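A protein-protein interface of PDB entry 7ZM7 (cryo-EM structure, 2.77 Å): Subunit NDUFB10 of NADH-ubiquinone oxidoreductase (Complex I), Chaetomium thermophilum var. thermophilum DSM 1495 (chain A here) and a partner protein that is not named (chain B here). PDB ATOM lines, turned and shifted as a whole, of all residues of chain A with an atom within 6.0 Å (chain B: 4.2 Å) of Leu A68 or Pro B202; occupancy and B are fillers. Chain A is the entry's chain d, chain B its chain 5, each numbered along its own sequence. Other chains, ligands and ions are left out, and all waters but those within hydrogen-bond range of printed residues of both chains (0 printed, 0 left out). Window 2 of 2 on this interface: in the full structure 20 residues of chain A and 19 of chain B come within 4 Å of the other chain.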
ATOM      1  N   GLY A  64     -16.462 -13.249 -11.622  1.00  0.00           N
ATOM      2  CA  GLY A  64     -16.521 -13.550 -13.032  1.00  0.00           C
ATOM      3  C   GLY A  64     -17.796 -13.092 -13.694  1.00  0.00           C
ATOM      4  O   GLY A  64     -17.975 -11.896 -13.915  1.00  0.00           O
ATOM      5  N   VAL A  65     -18.677 -14.026 -14.048  1.00  0.00           N
ATOM      6  CA  VAL A  65     -19.961 -13.626 -14.606  1.00  0.00           C
ATOM      7  C   VAL A  65     -20.820 -12.958 -13.537  1.00  0.00           C
ATOM      8  O   VAL A  65     -21.535 -11.987 -13.810  1.00  0.00           O
ATOM      9  CB  VAL A  65     -20.678 -14.824 -15.250  1.00  0.00           C
ATOM     10  CG1 VAL A  65     -21.002 -15.882 -14.232  1.00  0.00           C
ATOM     11  CG2 VAL A  65     -21.924 -14.361 -15.947  1.00  0.00           C
ATOM     12  N   ASN A  66     -20.736 -13.443 -12.301  1.00  0.00           N
ATOM     13  CA  ASN A  66     -21.531 -12.940 -11.195  1.00  0.00           C
ATOM     14  C   ASN A  66     -20.973 -11.663 -10.596  1.00  0.00           C
ATOM     15  O   ASN A  66     -21.405 -11.278  -9.512  1.00  0.00           O
ATOM     16  CB  ASN A  66     -21.654 -14.012 -10.111  1.00  0.00           C
ATOM     17  CG  ASN A  66     -22.321 -15.279 -10.612  1.00  0.00           C
ATOM     18  OD1 ASN A  66     -23.451 -15.252 -11.080  1.00  0.00           O
ATOM     19  ND2 ASN A  66     -21.614 -16.388 -10.531  1.00  0.00           N
ATOM     20  N   HIS A  67     -20.023 -10.991 -11.245  1.00  0.00           N
ATOM     21  CA  HIS A  67     -19.553  -9.715 -10.715  1.00  0.00           C
ATOM     22  C   HIS A  67     -20.662  -8.675 -10.663  1.00  0.00           C
ATOM     23  O   HIS A  67     -20.629  -7.800  -9.798  1.00  0.00           O
ATOM     24  CB  HIS A  67     -18.382  -9.177 -11.539  1.00  0.00           C
ATOM     25  CG  HIS A  67     -18.798  -8.410 -12.749  1.00  0.00           C
ATOM     26  ND1 HIS A  67     -18.870  -7.036 -12.771  1.00  0.00           N
ATOM     27  CD2 HIS A  67     -19.180  -8.825 -13.976  1.00  0.00           C
ATOM     28  CE1 HIS A  67     -19.279  -6.637 -13.961  1.00  0.00           C
ATOM     29  NE2 HIS A  67     -19.468  -7.703 -14.712  1.00  0.00           N
ATOM     30  N   LEU A  68     -21.660  -8.783 -11.523  1.00  0.00           N
ATOM     31  CA  LEU A  68     -22.715  -7.793 -11.640  1.00  0.00           C
ATOM     32  C   LEU A  68     -23.665  -7.786 -10.454  1.00  0.00           C
ATOM     33  O   LEU A  68     -24.545  -6.926 -10.389  1.00  0.00           O
ATOM     34  CB  LEU A  68     -23.498  -8.018 -12.935  1.00  0.00           C
ATOM     35  CG  LEU A  68     -22.994  -7.224 -14.130  1.00  0.00           C
ATOM     36  CD1 LEU A  68     -23.523  -7.745 -15.438  1.00  0.00           C
ATOM     37  CD2 LEU A  68     -23.426  -5.820 -13.936  1.00  0.00           C
ATOM     38  N   GLU A  69     -23.511  -8.718  -9.521  1.00  0.00           N
ATOM     39  CA  GLU A  69     -24.361  -8.782  -8.349  1.00  0.00           C
ATOM     40  C   GLU A  69     -23.604  -8.806  -7.041  1.00  0.00           C
ATOM     41  O   GLU A  69     -24.190  -8.458  -6.014  1.00  0.00           O
ATOM     42  CB  GLU A  69     -25.250 -10.023  -8.414  1.00  0.00           C
ATOM     43  CG  GLU A  69     -24.475 -11.309  -8.559  1.00  0.00           C
ATOM     44  CD  GLU A  69     -24.041 -11.884  -7.224  1.00  0.00           C
ATOM     45  OE1 GLU A  69     -24.672 -11.548  -6.198  1.00  0.00           O
ATOM     46  OE2 GLU A  69     -23.065 -12.662  -7.201  1.00  0.00           O
ATOM     47  N   LYS A  70     -22.334  -9.196  -7.029  1.00  0.00           N
ATOM     48  CA  LYS A  70     -21.642  -9.491  -5.789  1.00  0.00           C
ATOM     49  C   LYS A  70     -20.701  -8.381  -5.347  1.00  0.00           C
ATOM     50  O   LYS A  70     -20.242  -8.399  -4.202  1.00  0.00           O
ATOM     51  CB  LYS A  70     -20.866 -10.809  -5.942  1.00  0.00           C
ATOM     52  CG  LYS A  70     -20.232 -11.353  -4.675  1.00  0.00           C
ATOM     53  CD  LYS A  70     -21.296 -11.698  -3.649  1.00  0.00           C
ATOM     54  CE  LYS A  70     -22.180 -12.832  -4.136  1.00  0.00           C
ATOM     55  NZ  LYS A  70     -21.441 -14.118  -4.223  1.00  0.00           N
ATOM     56  N   CYS A  71     -20.432  -7.403  -6.207  1.00  0.00           N
ATOM     57  CA  CYS A  71     -19.415  -6.393  -5.940  1.00  0.00           C
ATOM     58  C   CYS A  71     -19.977  -4.971  -5.967  1.00  0.00           C
ATOM     59  O   CYS A  71     -19.234  -4.013  -6.180  1.00  0.00           O
ATOM     60  CB  CYS A  71     -18.263  -6.537  -6.935  1.00  0.00           C
ATOM     61  SG  CYS A  71     -17.704  -8.229  -7.222  1.00  0.00           S
ATOM     62  N   ARG A  75     -18.545  -1.176  -5.538  1.00  0.00           N
ATOM     63  CA  ARG A  75     -18.802  -0.242  -6.623  1.00  0.00           C
ATOM     64  C   ARG A  75     -19.339   1.074  -6.094  1.00  0.00           C
ATOM     65  O   ARG A  75     -18.924   2.146  -6.543  1.00  0.00           O
ATOM     66  CB  ARG A  75     -19.786  -0.843  -7.614  1.00  0.00           C
ATOM     67  CG  ARG A  75     -19.180  -1.797  -8.578  1.00  0.00           C
ATOM     68  CD  ARG A  75     -20.098  -2.001  -9.720  1.00  0.00           C
ATOM     69  NE  ARG A  75     -21.397  -2.476  -9.273  1.00  0.00           N
ATOM     70  CZ  ARG A  75     -21.810  -3.733  -9.372  1.00  0.00           C
ATOM     71  NH1 ARG A  75     -23.016  -4.060  -8.946  1.00  0.00           N
ATOM     72  NH2 ARG A  75     -21.022  -4.656  -9.899  1.00  0.00           N
ATOM     73  N   PHE B 198     -14.859  -2.668 -16.543  1.00  0.00           N
ATOM     74  CA  PHE B 198     -15.991  -3.535 -16.812  1.00  0.00           C
ATOM     75  C   PHE B 198     -16.899  -3.672 -15.601  1.00  0.00           C
ATOM     76  O   PHE B 198     -18.114  -3.792 -15.759  1.00  0.00           O
ATOM     77  CB  PHE B 198     -15.486  -4.891 -17.285  1.00  0.00           C
ATOM     78  CG  PHE B 198     -14.534  -4.804 -18.431  1.00  0.00           C
ATOM     79  CD1 PHE B 198     -14.624  -3.778 -19.350  1.00  0.00           C
ATOM     80  CD2 PHE B 198     -13.544  -5.746 -18.595  1.00  0.00           C
ATOM     81  CE1 PHE B 198     -13.740  -3.692 -20.388  1.00  0.00           C
ATOM     82  CE2 PHE B 198     -12.664  -5.657 -19.646  1.00  0.00           C
ATOM     83  CZ  PHE B 198     -12.768  -4.633 -20.537  1.00  0.00           C
ATOM     84  N   SER B 199     -16.349  -3.620 -14.392  1.00  0.00           N
ATOM     85  CA  SER B 199     -17.210  -3.621 -13.219  1.00  0.00           C
ATOM     86  C   SER B 199     -18.116  -2.399 -13.189  1.00  0.00           C
ATOM     87  O   SER B 199     -19.225  -2.467 -12.659  1.00  0.00           O
ATOM     88  CB  SER B 199     -16.375  -3.697 -11.950  1.00  0.00           C
ATOM     89  OG  SER B 199     -15.419  -2.666 -11.919  1.00  0.00           O
ATOM     90  N   LEU B 200     -17.681  -1.296 -13.776  1.00  0.00           N
ATOM     91  CA  LEU B 200     -18.392  -0.036 -13.678  1.00  0.00           C
ATOM     92  C   LEU B 200     -19.207   0.319 -14.903  1.00  0.00           C
ATOM     93  O   LEU B 200     -20.045   1.214 -14.812  1.00  0.00           O
ATOM     94  CB  LEU B 200     -17.409   1.098 -13.417  1.00  0.00           C
ATOM     95  CG  LEU B 200     -16.859   1.164 -12.011  1.00  0.00           C
ATOM     96  CD1 LEU B 200     -15.975   2.355 -11.942  1.00  0.00           C
ATOM     97  CD2 LEU B 200     -17.989   1.282 -11.034  1.00  0.00           C
ATOM     98  N   ALA B 201     -18.985  -0.348 -16.032  1.00  0.00           N
ATOM     99  CA  ALA B 201     -19.586   0.086 -17.291  1.00  0.00           C
ATOM    100  C   ALA B 201     -21.113   0.153 -17.303  1.00  0.00           C
ATOM    101  O   ALA B 201     -21.646   1.116 -17.880  1.00  0.00           O
ATOM    102  CB  ALA B 201     -19.090  -0.808 -18.430  1.00  0.00           C
ATOM    103  N   PRO B 202     -21.900  -0.820 -16.765  1.00  0.00           N
ATOM    104  CA  PRO B 202     -23.364  -0.758 -16.898  1.00  0.00           C
ATOM    105  C   PRO B 202     -23.971   0.564 -16.411  1.00  0.00           C
ATOM    106  O   PRO B 202     -25.014   0.929 -16.907  1.00  0.00           O
ATOM    107  CB  PRO B 202     -23.891  -1.858 -15.970  1.00  0.00           C
ATOM    108  CG  PRO B 202     -22.765  -2.848 -15.866  1.00  0.00           C
ATOM    109  CD  PRO B 202     -21.505  -2.027 -16.002  1.00  0.00           C
ATOM    110  N   TYR B 203     -23.316   1.239 -15.465  1.00  0.00           N
ATOM    111  CA  TYR B 203     -23.890   2.465 -14.853  1.00  0.00           C
ATOM    112  C   TYR B 203     -23.345   3.738 -15.500  1.00  0.00           C
ATOM    113  O   TYR B 203     -23.836   4.817 -15.158  1.00  0.00           O
ATOM    114  CB  TYR B 203     -23.568   2.420 -13.360  1.00  0.00           C
ATOM    115  CG  TYR B 203     -23.560   1.007 -12.840  1.00  0.00           C
ATOM    116  CD1 TYR B 203     -24.745   0.323 -12.648  1.00  0.00           C
ATOM    117  CD2 TYR B 203     -22.375   0.335 -12.592  1.00  0.00           C
ATOM    118  CE1 TYR B 203     -24.764  -0.984 -12.198  1.00  0.00           C
ATOM    119  CE2 TYR B 203     -22.374  -0.976 -12.148  1.00  0.00           C
ATOM    120  CZ  TYR B 203     -23.573  -1.634 -11.945  1.00  0.00           C
ATOM    121  OH  TYR B 203     -23.592  -2.923 -11.508  1.00  0.00           O
ATOM    122  N   ILE B 204     -22.388   3.619 -16.418  1.00  0.00           N
ATOM    123  CA  ILE B 204     -21.732   4.832 -16.994  1.00  0.00           C
ATOM    124  C   ILE B 204     -22.694   5.558 -17.942  1.00  0.00           C
ATOM    125  O   ILE B 204     -23.561   4.886 -18.527  1.00  0.00           O
ATOM    126  CB  ILE B 204     -20.379   4.452 -17.629  1.00  0.00           C
ATOM    127  CG1 ILE B 204     -19.420   3.933 -16.557  1.00  0.00           C
ATOM    128  CG2 ILE B 204     -19.757   5.601 -18.409  1.00  0.00           C
ATOM    129  CD1 ILE B 204     -19.507   4.697 -15.256  1.00  0.00           C
ATOM    130  N   TYR B 269     -22.636  -2.054 -24.002  1.00  0.00           N
ATOM    131  CA  TYR B 269     -23.519  -1.062 -23.420  1.00  0.00           C
ATOM    132  C   TYR B 269     -23.713   0.137 -24.325  1.00  0.00           C
ATOM    133  O   TYR B 269     -24.048   1.222 -23.849  1.00  0.00           O
ATOM    134  CB  TYR B 269     -22.999  -0.646 -22.048  1.00  0.00           C
ATOM    135  CG  TYR B 269     -23.283  -1.698 -21.013  1.00  0.00           C
ATOM    136  CD1 TYR B 269     -24.551  -1.859 -20.504  1.00  0.00           C
ATOM    137  CD2 TYR B 269     -22.283  -2.547 -20.559  1.00  0.00           C
ATOM    138  CE1 TYR B 269     -24.825  -2.828 -19.581  1.00  0.00           C
ATOM    139  CE2 TYR B 269     -22.548  -3.517 -19.627  1.00  0.00           C
ATOM    140  CZ  TYR B 269     -23.821  -3.656 -19.148  1.00  0.00           C
ATOM    141  OH  TYR B 269     -24.089  -4.621 -18.218  1.00  0.00           O
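OH of Tyr B203 is in hydrogen-bond range of NH1 of Arg A75, 2.9 Å away.
The backbone carbonyl oxygen (O) of His A67 is in hydrogen-bond range of the guanidinium group (NH2) of Arg A75 (3.2 Å).
His A67 touches Phe B198.
His A67 touches Ser B199 (CE1 to CA, 3.7 Å).
Pro B202 touches Leu A68.
Leu A68 touches Tyr B203 (CD2 to OH, 3.8 Å).
CD of Arg A75 touches O of Ser B199, at 3.1 Å.
Asn A66 touches none of the printed residues of chain B.
Of the printed residues of chain B, Leu A68 touches Pro B202 and Tyr B203.
Printed residues of chain B within 4 Å of Arg A75: Ser B199 and Tyr B203.
Printed residues of chain A within 4 Å of Phe B198: His A67 (3.6 Å).
Of the printed residues of chain A, Ser B199 touches His A67 (3.7 Å) and Arg A75 (3.1 Å).
Ala B201 touches none of the printed residues of chain A.
Of the printed residues of chain A, Pro B202 touches Leu A68 (3.6 Å).
Of the printed residues of chain A, Tyr B203 touches Leu A68 (3.8 Å) and Arg A75 (2.9 Å).
The nearest printed residue of chain B that does not touch Leu A68 is Tyr B269 (4.2 Å).
The nearest residue of chain A that does not touch Pro B202 is His A67 (5.5 Å).
Of the 8 printed residues of chain B, 4 touch a printed residue of chain A.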
